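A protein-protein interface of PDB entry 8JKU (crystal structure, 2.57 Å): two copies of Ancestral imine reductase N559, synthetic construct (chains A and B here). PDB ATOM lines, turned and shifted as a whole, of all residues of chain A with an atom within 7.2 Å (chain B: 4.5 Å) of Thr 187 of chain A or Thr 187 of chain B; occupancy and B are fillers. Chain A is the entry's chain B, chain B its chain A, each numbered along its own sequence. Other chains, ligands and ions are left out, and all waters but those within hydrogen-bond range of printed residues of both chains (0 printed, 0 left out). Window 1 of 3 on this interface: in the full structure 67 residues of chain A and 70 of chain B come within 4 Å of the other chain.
Of the printed residues of chain B, Thr 187 of chain A touches Thr 187 (3.2 Å) and Gly 191 (3.6 Å).
Thr 187 of chain B touches just these residues of chain A: Thr 187, Gly 191 and Val 269.
Printed residues of chain A within 4 Å of Val 269 of chain B: Ser 190.
Printed residues of chain A within 4 Å of Ser 190 of chain B: Val 269 (3.6 Å) and Phe 286 (3.5 Å).
Phe 185 of chain B touches none of the printed residues of chain A.
The nearest printed residue of chain B that does not touch Thr 187 of chain A is Val 269 of chain B (4.004 Å).
The nearest printed residue of chain A that does not touch Thr 188 of chain B is Leu 184 of chain A (4.1 Å).
The backbone carbonyl oxygen (O) of Asp 183 of chain B lies within hydrogen-bond range of the side-chain hydroxyl (OG1) of Thr 187 of chain B, 2.9 Å away.
The backbone carbonyl oxygen of Leu 184 of chain B lies within hydrogen-bond range of the side-chain hydroxyl of Thr 188 of chain B, 2.6 Å away.
The side-chain hydroxyl of Ser 190 of chain B lies within hydrogen-bond range of the backbone carbonyl oxygen of Trp 186 of chain B (2.8 Å).
O of Asp 183 of chain A is in hydrogen-bond range of OG1 of Thr 187 of chain A, at 2.7 Å.
OG1 of Thr 188 of chain A lies within hydrogen-bond range of O of Leu 184 of chain A.
O of Trp 186 of chain A lies within hydrogen-bond range of OG of Ser 190 of chain A (3.1 Å).
O of Thr 187 of chain B touches CG2 of Thr 187 of chain A, at 3.2 Å.
Thr 187 of chain A touches Gly 191 of chain B.
CG2 of Thr 188 of chain B touches OG1 of Thr 188 of chain A, at 3.2 Å.
Gly 191 of chain A touches Leu 184 of chain B (C to CD1, 3.7 Å).
Thr 187 of chain B touches Gly 191 of chain A (CG2 to CA, 3.5 Å).
Tyr 192 of chain A touches Leu 184 of chain B (N to CD1, 3.3 Å).
Trp 186 of chain B touches Ile 249 of chain A.
CD1 of Ile 252 of chain A touches N of Asp 183 of chain B (3.6 Å).
Thr 187 of chain B touches Val 269 of chain A.
Trp 186 of chain B touches Phe 286 of chain A.
Thr 187 of chain A touches its own counterpart, Thr 187 of chain B.
Thr 188 of chain A touches its own counterpart, Thr 188 of chain B.
Gly 191 of chain A touches Asp 183 of chain B, but with the chains exchanged Asp 183 of chain A does not touch Gly 191 of chain B (4.4 Å).
Gly 191 of chain A touches Leu 184 of chain B, but with the chains exchanged Leu 184 of chain A does not touch Gly 191 of chain B (4.1 Å).
Of the 17 pairs that touch across the chains among the printed residues, 6 have their exchanged pair printed and touching as well.
Of the 11 printed residues of chain B, 9 touch a printed residue of chain A.
Hydrophobic or aromatic side chains of chain B within 4 Å of the printed part of chain A: Leu 184, Trp 186, Met 189 and Val 269.
OD2 of Asp 183 of chain B lies within hydrogen-bond range of ND1 of His 194 of chain A (2.4 Å).
O of Gly 191 of chain A sits close to OD1 of Asp 183 of chain B (3.5 Å).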
ATOM      1  N   LEU A 181     -21.015 -25.449   7.603  1.00  0.00           N
ATOM      2  CA  LEU A 181     -19.678 -25.540   8.177  1.00  0.00           C
ATOM      3  C   LEU A 181     -18.623 -25.733   7.096  1.00  0.00           C
ATOM      4  O   LEU A 181     -17.504 -25.222   7.226  1.00  0.00           O
ATOM      5  CB  LEU A 181     -19.619 -26.678   9.195  1.00  0.00           C
ATOM      6  CG  LEU A 181     -20.369 -26.417  10.503  1.00  0.00           C
ATOM      7  CD1 LEU A 181     -20.604 -27.718  11.255  1.00  0.00           C
ATOM      8  CD2 LEU A 181     -19.617 -25.420  11.373  1.00  0.00           C
ATOM      9  N   LEU A 182     -18.957 -26.458   6.024  1.00  0.00           N
ATOM     10  CA  LEU A 182     -18.033 -26.584   4.903  1.00  0.00           C
ATOM     11  C   LEU A 182     -17.946 -25.284   4.109  1.00  0.00           C
ATOM     12  O   LEU A 182     -16.877 -24.950   3.584  1.00  0.00           O
ATOM     13  CB  LEU A 182     -18.463 -27.733   3.992  1.00  0.00           C
ATOM     14  CG  LEU A 182     -18.533 -29.115   4.644  1.00  0.00           C
ATOM     15  CD1 LEU A 182     -19.458 -30.040   3.863  1.00  0.00           C
ATOM     16  CD2 LEU A 182     -17.145 -29.727   4.763  1.00  0.00           C
ATOM     17  N   ASP A 183     -19.055 -24.549   4.004  1.00  0.00           N
ATOM     18  CA  ASP A 183     -19.012 -23.217   3.408  1.00  0.00           C
ATOM     19  C   ASP A 183     -18.013 -22.332   4.142  1.00  0.00           C
ATOM     20  O   ASP A 183     -17.186 -21.655   3.520  1.00  0.00           O
ATOM     21  CB  ASP A 183     -20.412 -22.598   3.431  1.00  0.00           C
ATOM     22  CG  ASP A 183     -20.507 -21.322   2.613  1.00  0.00           C
ATOM     23  OD1 ASP A 183     -19.590 -21.046   1.810  1.00  0.00           O
ATOM     24  OD2 ASP A 183     -21.510 -20.593   2.774  1.00  0.00           O
ATOM     25  N   LEU A 184     -18.067 -22.336   5.475  1.00  0.00           N
ATOM     26  CA  LEU A 184     -17.121 -21.552   6.261  1.00  0.00           C
ATOM     27  C   LEU A 184     -15.701 -22.077   6.087  1.00  0.00           C
ATOM     28  O   LEU A 184     -14.765 -21.301   5.865  1.00  0.00           O
ATOM     29  CB  LEU A 184     -17.537 -21.572   7.733  1.00  0.00           C
ATOM     30  CG  LEU A 184     -16.522 -21.131   8.788  1.00  0.00           C
ATOM     31  CD1 LEU A 184     -16.242 -19.642   8.685  1.00  0.00           C
ATOM     32  CD2 LEU A 184     -17.025 -21.481  10.185  1.00  0.00           C
ATOM     33  N   PHE A 185     -15.527 -23.396   6.165  1.00  0.00           N
ATOM     34  CA  PHE A 185     -14.188 -23.975   6.114  1.00  0.00           C
ATOM     35  C   PHE A 185     -13.492 -23.656   4.796  1.00  0.00           C
ATOM     36  O   PHE A 185     -12.367 -23.146   4.782  1.00  0.00           O
ATOM     37  CB  PHE A 185     -14.272 -25.488   6.327  1.00  0.00           C
ATOM     38  CG  PHE A 185     -12.940 -26.184   6.293  1.00  0.00           C
ATOM     39  CD1 PHE A 185     -12.391 -26.601   5.090  1.00  0.00           C
ATOM     40  CD2 PHE A 185     -12.242 -26.427   7.462  1.00  0.00           C
ATOM     41  CE1 PHE A 185     -11.167 -27.240   5.056  1.00  0.00           C
ATOM     42  CE2 PHE A 185     -11.019 -27.068   7.433  1.00  0.00           C
ATOM     43  CZ  PHE A 185     -10.481 -27.473   6.229  1.00  0.00           C
ATOM     44  N   TRP A 186     -14.145 -23.957   3.671  1.00  0.00           N
ATOM     45  CA  TRP A 186     -13.491 -23.782   2.378  1.00  0.00           C
ATOM     46  C   TRP A 186     -13.313 -22.305   2.040  1.00  0.00           C
ATOM     47  O   TRP A 186     -12.312 -21.921   1.426  1.00  0.00           O
ATOM     48  CB  TRP A 186     -14.285 -24.498   1.287  1.00  0.00           C
ATOM     49  CG  TRP A 186     -14.191 -25.992   1.375  1.00  0.00           C
ATOM     50  CD1 TRP A 186     -15.227 -26.877   1.425  1.00  0.00           C
ATOM     51  CD2 TRP A 186     -12.991 -26.775   1.429  1.00  0.00           C
ATOM     52  NE1 TRP A 186     -14.748 -28.163   1.506  1.00  0.00           N
ATOM     53  CE2 TRP A 186     -13.379 -28.127   1.510  1.00  0.00           C
ATOM     54  CE3 TRP A 186     -11.627 -26.465   1.416  1.00  0.00           C
ATOM     55  CZ2 TRP A 186     -12.453 -29.167   1.577  1.00  0.00           C
ATOM     56  CZ3 TRP A 186     -10.710 -27.498   1.483  1.00  0.00           C
ATOM     57  CH2 TRP A 186     -11.126 -28.833   1.563  1.00  0.00           C
ATOM     58  N   THR A 187     -14.275 -21.461   2.422  1.00  0.00           N
ATOM     59  CA  THR A 187     -14.100 -20.025   2.225  1.00  0.00           C
ATOM     60  C   THR A 187     -12.892 -19.519   3.004  1.00  0.00           C
ATOM     61  O   THR A 187     -12.088 -18.738   2.481  1.00  0.00           O
ATOM     62  CB  THR A 187     -15.366 -19.273   2.642  1.00  0.00           C
ATOM     63  OG1 THR A 187     -16.471 -19.713   1.840  1.00  0.00           O
ATOM     64  CG2 THR A 187     -15.186 -17.770   2.466  1.00  0.00           C
ATOM     65  N   THR A 188     -12.742 -19.965   4.253  1.00  0.00           N
ATOM     66  CA  THR A 188     -11.576 -19.578   5.039  1.00  0.00           C
ATOM     67  C   THR A 188     -10.292 -20.100   4.408  1.00  0.00           C
ATOM     68  O   THR A 188      -9.286 -19.382   4.342  1.00  0.00           O
ATOM     69  CB  THR A 188     -11.713 -20.093   6.472  1.00  0.00           C
ATOM     70  OG1 THR A 188     -12.929 -19.598   7.045  1.00  0.00           O
ATOM     71  CG2 THR A 188     -10.533 -19.640   7.320  1.00  0.00           C
ATOM     72  N   MET A 189     -10.305 -21.351   3.943  1.00  0.00           N
ATOM     73  CA  MET A 189      -9.140 -21.898   3.253  1.00  0.00           C
ATOM     74  C   MET A 189      -8.765 -21.032   2.058  1.00  0.00           C
ATOM     75  O   MET A 189      -7.590 -20.702   1.855  1.00  0.00           O
ATOM     76  CB  MET A 189      -9.423 -23.329   2.796  1.00  0.00           C
ATOM     77  CG  MET A 189      -9.526 -24.340   3.916  1.00  0.00           C
ATOM     78  SD  MET A 189      -7.992 -24.498   4.846  1.00  0.00           S
ATOM     79  CE  MET A 189      -8.591 -24.189   6.505  1.00  0.00           C
ATOM     80  N   SER A 190      -9.757 -20.662   1.247  1.00  0.00           N
ATOM     81  CA  SER A 190      -9.479 -19.875   0.053  1.00  0.00           C
ATOM     82  C   SER A 190      -8.846 -18.539   0.417  1.00  0.00           C
ATOM     83  O   SER A 190      -7.905 -18.088  -0.246  1.00  0.00           O
ATOM     84  CB  SER A 190     -10.767 -19.666  -0.744  1.00  0.00           C
ATOM     85  OG  SER A 190     -11.214 -20.888  -1.313  1.00  0.00           O
ATOM     86  N   GLY A 191      -9.339 -17.900   1.479  1.00  0.00           N
ATOM     87  CA  GLY A 191      -8.776 -16.625   1.884  1.00  0.00           C
ATOM     88  C   GLY A 191      -7.349 -16.748   2.380  1.00  0.00           C
ATOM     89  O   GLY A 191      -6.515 -15.875   2.123  1.00  0.00           O
ATOM     90  N   TYR A 192      -7.048 -17.831   3.098  1.00  0.00           N
ATOM     91  CA  TYR A 192      -5.692 -18.029   3.598  1.00  0.00           C
ATOM     92  C   TYR A 192      -4.710 -18.225   2.453  1.00  0.00           C
ATOM     93  O   TYR A 192      -3.620 -17.640   2.453  1.00  0.00           O
ATOM     94  CB  TYR A 192      -5.654 -19.226   4.546  1.00  0.00           C
ATOM     95  CG  TYR A 192      -4.283 -19.529   5.098  1.00  0.00           C
ATOM     96  CD1 TYR A 192      -3.640 -18.634   5.938  1.00  0.00           C
ATOM     97  CD2 TYR A 192      -3.630 -20.713   4.779  1.00  0.00           C
ATOM     98  CE1 TYR A 192      -2.385 -18.906   6.446  1.00  0.00           C
ATOM     99  CE2 TYR A 192      -2.375 -20.995   5.285  1.00  0.00           C
ATOM    100  CZ  TYR A 192      -1.758 -20.087   6.120  1.00  0.00           C
ATOM    101  OH  TYR A 192      -0.509 -20.356   6.629  1.00  0.00           O
ATOM    102  N   LEU A 193      -5.073 -19.048   1.468  1.00  0.00           N
ATOM    103  CA  LEU A 193      -4.192 -19.250   0.324  1.00  0.00           C
ATOM    104  C   LEU A 193      -3.960 -17.941  -0.422  1.00  0.00           C
ATOM    105  O   LEU A 193      -2.836 -17.650  -0.847  1.00  0.00           O
ATOM    106  CB  LEU A 193      -4.781 -20.309  -0.607  1.00  0.00           C
ATOM    107  CG  LEU A 193      -4.773 -21.738  -0.058  1.00  0.00           C
ATOM    108  CD1 LEU A 193      -5.444 -22.689  -1.040  1.00  0.00           C
ATOM    109  CD2 LEU A 193      -3.355 -22.205   0.251  1.00  0.00           C
ATOM    110  N   HIS A 194      -5.010 -17.130  -0.577  1.00  0.00           N
ATOM    111  CA  HIS A 194      -4.855 -15.851  -1.261  1.00  0.00           C
ATOM    112  C   HIS A 194      -3.946 -14.912  -0.478  1.00  0.00           C
ATOM    113  O   HIS A 194      -3.135 -14.190  -1.068  1.00  0.00           O
ATOM    114  CB  HIS A 194      -6.223 -15.208  -1.484  1.00  0.00           C
ATOM    115  CG  HIS A 194      -6.195 -14.048  -2.429  1.00  0.00           C
ATOM    116  ND1 HIS A 194      -5.595 -12.848  -2.115  1.00  0.00           N
ATOM    117  CD2 HIS A 194      -6.693 -13.905  -3.680  1.00  0.00           C
ATOM    118  CE1 HIS A 194      -5.724 -12.015  -3.132  1.00  0.00           C
ATOM    119  NE2 HIS A 194      -6.386 -12.631  -4.095  1.00  0.00           N
ATOM    120  N   ILE A 249     -10.755  -3.397   1.685  1.00  0.00           N
ATOM    121  CA  ILE A 249     -10.878  -4.432   0.665  1.00  0.00           C
ATOM    122  C   ILE A 249     -10.449  -3.889  -0.691  1.00  0.00           C
ATOM    123  O   ILE A 249      -9.921  -4.631  -1.528  1.00  0.00           O
ATOM    124  CB  ILE A 249     -12.317  -4.980   0.634  1.00  0.00           C
ATOM    125  CG1 ILE A 249     -12.609  -5.752   1.923  1.00  0.00           C
ATOM    126  CG2 ILE A 249     -12.524  -5.876  -0.579  1.00  0.00           C
ATOM    127  CD1 ILE A 249     -14.038  -5.633   2.402  1.00  0.00           C
ATOM    128  N   ILE A 252      -6.785  -4.259  -0.709  1.00  0.00           N
ATOM    129  CA  ILE A 252      -6.403  -5.646  -0.952  1.00  0.00           C
ATOM    130  C   ILE A 252      -6.415  -5.942  -2.444  1.00  0.00           C
ATOM    131  O   ILE A 252      -5.521  -6.620  -2.967  1.00  0.00           O
ATOM    132  CB  ILE A 252      -7.336  -6.599  -0.183  1.00  0.00           C
ATOM    133  CG1 ILE A 252      -7.135  -6.441   1.325  1.00  0.00           C
ATOM    134  CG2 ILE A 252      -7.094  -8.042  -0.599  1.00  0.00           C
ATOM    135  CD1 ILE A 252      -8.358  -6.797   2.140  1.00  0.00           C
ATOM    136  N   LEU A 265     -11.244 -13.729  -5.926  1.00  0.00           N
ATOM    137  CA  LEU A 265     -11.828 -13.951  -4.605  1.00  0.00           C
ATOM    138  C   LEU A 265     -12.014 -12.663  -3.817  1.00  0.00           C
ATOM    139  O   LEU A 265     -13.132 -12.420  -3.329  1.00  0.00           O
ATOM    140  CB  LEU A 265     -10.965 -14.949  -3.829  1.00  0.00           C
ATOM    141  CG  LEU A 265     -11.541 -15.414  -2.490  1.00  0.00           C
ATOM    142  CD1 LEU A 265     -12.887 -16.087  -2.690  1.00  0.00           C
ATOM    143  CD2 LEU A 265     -10.564 -16.344  -1.789  1.00  0.00           C
ATOM    144  N   PRO A 266     -10.997 -11.815  -3.636  1.00  0.00           N
ATOM    145  CA  PRO A 266     -11.240 -10.562  -2.894  1.00  0.00           C
ATOM    146  C   PRO A 266     -12.286  -9.680  -3.553  1.00  0.00           C
ATOM    147  O   PRO A 266     -13.059  -9.008  -2.857  1.00  0.00           O
ATOM    148  CB  PRO A 266      -9.855  -9.893  -2.858  1.00  0.00           C
ATOM    149  CG  PRO A 266      -9.079 -10.533  -3.974  1.00  0.00           C
ATOM    150  CD  PRO A 266      -9.597 -11.944  -4.082  1.00  0.00           C
ATOM    151  N   VAL A 269     -15.603 -10.732  -2.417  1.00  0.00           N
ATOM    152  CA  VAL A 269     -15.896 -10.143  -1.114  1.00  0.00           C
ATOM    153  C   VAL A 269     -16.302  -8.683  -1.275  1.00  0.00           C
ATOM    154  O   VAL A 269     -17.193  -8.189  -0.572  1.00  0.00           O
ATOM    155  CB  VAL A 269     -14.682 -10.290  -0.176  1.00  0.00           C
ATOM    156  CG1 VAL A 269     -14.933  -9.563   1.139  1.00  0.00           C
ATOM    157  CG2 VAL A 269     -14.362 -11.762   0.059  1.00  0.00           C
ATOM    158  N   PHE A 286     -19.817  -4.758   9.366  1.00  0.00           N
ATOM    159  CA  PHE A 286     -19.630  -5.763   8.326  1.00  0.00           C
ATOM    160  C   PHE A 286     -20.607  -6.916   8.508  1.00  0.00           C
ATOM    161  O   PHE A 286     -21.043  -7.525   7.524  1.00  0.00           O
ATOM    162  CB  PHE A 286     -18.192  -6.279   8.336  1.00  0.00           C
ATOM    163  CG  PHE A 286     -17.837  -7.105   7.127  1.00  0.00           C
ATOM    164  CD1 PHE A 286     -18.034  -8.476   7.125  1.00  0.00           C
ATOM    165  CD2 PHE A 286     -17.310  -6.509   5.994  1.00  0.00           C
ATOM    166  CE1 PHE A 286     -17.712  -9.236   6.017  1.00  0.00           C
ATOM    167  CE2 PHE A 286     -16.984  -7.265   4.882  1.00  0.00           C
ATOM    168  CZ  PHE A 286     -17.185  -8.630   4.895  1.00  0.00           C
ATOM    169  N   ASP B 183      -7.044  -9.475   4.084  1.00  0.00           N
ATOM    170  CA  ASP B 183      -7.605 -10.362   3.068  1.00  0.00           C
ATOM    171  C   ASP B 183      -8.150 -11.629   3.713  1.00  0.00           C
ATOM    172  O   ASP B 183      -9.262 -12.073   3.403  1.00  0.00           O
ATOM    173  CB  ASP B 183      -6.527 -10.674   2.023  1.00  0.00           C
ATOM    174  CG  ASP B 183      -6.876 -11.849   1.113  1.00  0.00           C
ATOM    175  OD1 ASP B 183      -7.723 -12.699   1.459  1.00  0.00           O
ATOM    176  OD2 ASP B 183      -6.271 -11.931   0.024  1.00  0.00           O
ATOM    177  N   LEU B 184      -7.370 -12.231   4.608  1.00  0.00           N
ATOM    178  CA  LEU B 184      -7.810 -13.449   5.277  1.00  0.00           C
ATOM    179  C   LEU B 184      -8.985 -13.181   6.206  1.00  0.00           C
ATOM    180  O   LEU B 184      -9.943 -13.960   6.242  1.00  0.00           O
ATOM    181  CB  LEU B 184      -6.646 -14.048   6.058  1.00  0.00           C
ATOM    182  CG  LEU B 184      -6.945 -15.258   6.939  1.00  0.00           C
ATOM    183  CD1 LEU B 184      -7.436 -16.415   6.098  1.00  0.00           C
ATOM    184  CD2 LEU B 184      -5.695 -15.626   7.724  1.00  0.00           C
ATOM    185  N   PHE B 185      -8.929 -12.083   6.962  1.00  0.00           N
ATOM    186  CA  PHE B 185      -9.954 -11.816   7.965  1.00  0.00           C
ATOM    187  C   PHE B 185     -11.318 -11.580   7.324  1.00  0.00           C
ATOM    188  O   PHE B 185     -12.321 -12.169   7.740  1.00  0.00           O
ATOM    189  CB  PHE B 185      -9.547 -10.612   8.814  1.00  0.00           C
ATOM    190  CG  PHE B 185     -10.542 -10.263   9.881  1.00  0.00           C
ATOM    191  CD1 PHE B 185     -10.571 -10.968  11.071  1.00  0.00           C
ATOM    192  CD2 PHE B 185     -11.451  -9.237   9.693  1.00  0.00           C
ATOM    193  CE1 PHE B 185     -11.484 -10.655  12.054  1.00  0.00           C
ATOM    194  CE2 PHE B 185     -12.367  -8.920  10.672  1.00  0.00           C
ATOM    195  CZ  PHE B 185     -12.383  -9.630  11.855  1.00  0.00           C
ATOM    196  N   TRP B 186     -11.379 -10.705   6.317  1.00  0.00           N
ATOM    197  CA  TRP B 186     -12.670 -10.379   5.718  1.00  0.00           C
ATOM    198  C   TRP B 186     -13.212 -11.534   4.884  1.00  0.00           C
ATOM    199  O   TRP B 186     -14.431 -11.725   4.815  1.00  0.00           O
ATOM    200  CB  TRP B 186     -12.559  -9.117   4.858  1.00  0.00           C
ATOM    201  CG  TRP B 186     -12.266  -7.871   5.642  1.00  0.00           C
ATOM    202  CD1 TRP B 186     -11.278  -6.963   5.395  1.00  0.00           C
ATOM    203  CD2 TRP B 186     -12.965  -7.397   6.800  1.00  0.00           C
ATOM    204  NE1 TRP B 186     -11.317  -5.955   6.326  1.00  0.00           N
ATOM    205  CE2 TRP B 186     -12.345  -6.197   7.200  1.00  0.00           C
ATOM    206  CE3 TRP B 186     -14.055  -7.870   7.537  1.00  0.00           C
ATOM    207  CZ2 TRP B 186     -12.776  -5.464   8.303  1.00  0.00           C
ATOM    208  CZ3 TRP B 186     -14.482  -7.142   8.633  1.00  0.00           C
ATOM    209  CH2 TRP B 186     -13.844  -5.952   9.004  1.00  0.00           C
ATOM    210  N   THR B 187     -12.333 -12.306   4.238  1.00  0.00           N
ATOM    211  CA  THR B 187     -12.794 -13.482   3.506  1.00  0.00           C
ATOM    212  C   THR B 187     -13.362 -14.526   4.459  1.00  0.00           C
ATOM    213  O   THR B 187     -14.393 -15.145   4.169  1.00  0.00           O
ATOM    214  CB  THR B 187     -11.654 -14.072   2.675  1.00  0.00           C
ATOM    215  OG1 THR B 187     -11.263 -13.131   1.664  1.00  0.00           O
ATOM    216  CG2 THR B 187     -12.087 -15.378   2.013  1.00  0.00           C
ATOM    217  N   THR B 188     -12.707 -14.729   5.607  1.00  0.00           N
ATOM    218  CA  THR B 188     -13.262 -15.612   6.629  1.00  0.00           C
ATOM    219  C   THR B 188     -14.557 -15.041   7.191  1.00  0.00           C
ATOM    220  O   THR B 188     -15.523 -15.779   7.423  1.00  0.00           O
ATOM    221  CB  THR B 188     -12.246 -15.824   7.751  1.00  0.00           C
ATOM    222  OG1 THR B 188     -10.978 -16.188   7.195  1.00  0.00           O
ATOM    223  CG2 THR B 188     -12.714 -16.920   8.702  1.00  0.00           C
ATOM    224  N   MET B 189     -14.588 -13.727   7.426  1.00  0.00           N
ATOM    225  CA  MET B 189     -15.812 -13.063   7.863  1.00  0.00           C
ATOM    226  C   MET B 189     -16.975 -13.398   6.937  1.00  0.00           C
ATOM    227  O   MET B 189     -18.064 -13.771   7.390  1.00  0.00           O
ATOM    228  CB  MET B 189     -15.588 -11.549   7.894  1.00  0.00           C
ATOM    229  CG  MET B 189     -15.258 -10.963   9.256  1.00  0.00           C
ATOM    230  SD  MET B 189     -16.341 -11.539  10.565  1.00  0.00           S
ATOM    231  CE  MET B 189     -15.159 -11.925  11.851  1.00  0.00           C
ATOM    232  N   SER B 190     -16.758 -13.263   5.628  1.00  0.00           N
ATOM    233  CA  SER B 190     -17.842 -13.466   4.673  1.00  0.00           C
ATOM    234  C   SER B 190     -18.303 -14.918   4.666  1.00  0.00           C
ATOM    235  O   SER B 190     -19.494 -15.196   4.484  1.00  0.00           O
ATOM    236  CB  SER B 190     -17.394 -13.035   3.276  1.00  0.00           C
ATOM    237  OG  SER B 190     -16.835 -11.734   3.304  1.00  0.00           O
ATOM    238  N   GLY B 191     -17.376 -15.858   4.850  1.00  0.00           N
ATOM    239  CA  GLY B 191     -17.766 -17.258   4.909  1.00  0.00           C
ATOM    240  C   GLY B 191     -18.630 -17.567   6.116  1.00  0.00           C
ATOM    241  O   GLY B 191     -19.618 -18.300   6.013  1.00  0.00           O
ATOM    242  N   LEU B 265     -20.642 -15.738  -3.234  1.00  0.00           N
ATOM    243  CA  LEU B 265     -19.389 -16.131  -2.587  1.00  0.00           C
ATOM    244  C   LEU B 265     -19.045 -17.592  -2.829  1.00  0.00           C
ATOM    245  O   LEU B 265     -17.936 -17.877  -3.319  1.00  0.00           O
ATOM    246  CB  LEU B 265     -19.477 -15.818  -1.092  1.00  0.00           C
ATOM    247  CG  LEU B 265     -18.144 -15.686  -0.357  1.00  0.00           C
ATOM    248  CD1 LEU B 265     -17.343 -14.517  -0.905  1.00  0.00           C
ATOM    249  CD2 LEU B 265     -18.387 -15.531   1.140  1.00  0.00           C
ATOM    250  N   VAL B 269     -15.557 -19.202  -4.672  1.00  0.00           N
ATOM    251  CA  VAL B 269     -14.658 -20.255  -4.212  1.00  0.00           C
ATOM    252  C   VAL B 269     -14.684 -21.432  -5.174  1.00  0.00           C
ATOM    253  O   VAL B 269     -13.659 -22.091  -5.390  1.00  0.00           O
ATOM    254  CB  VAL B 269     -15.036 -20.686  -2.780  1.00  0.00           C
ATOM    255  CG1 VAL B 269     -14.232 -21.908  -2.360  1.00  0.00           C
ATOM    256  CG2 VAL B 269     -14.827 -19.534  -1.806  1.00  0.00           C
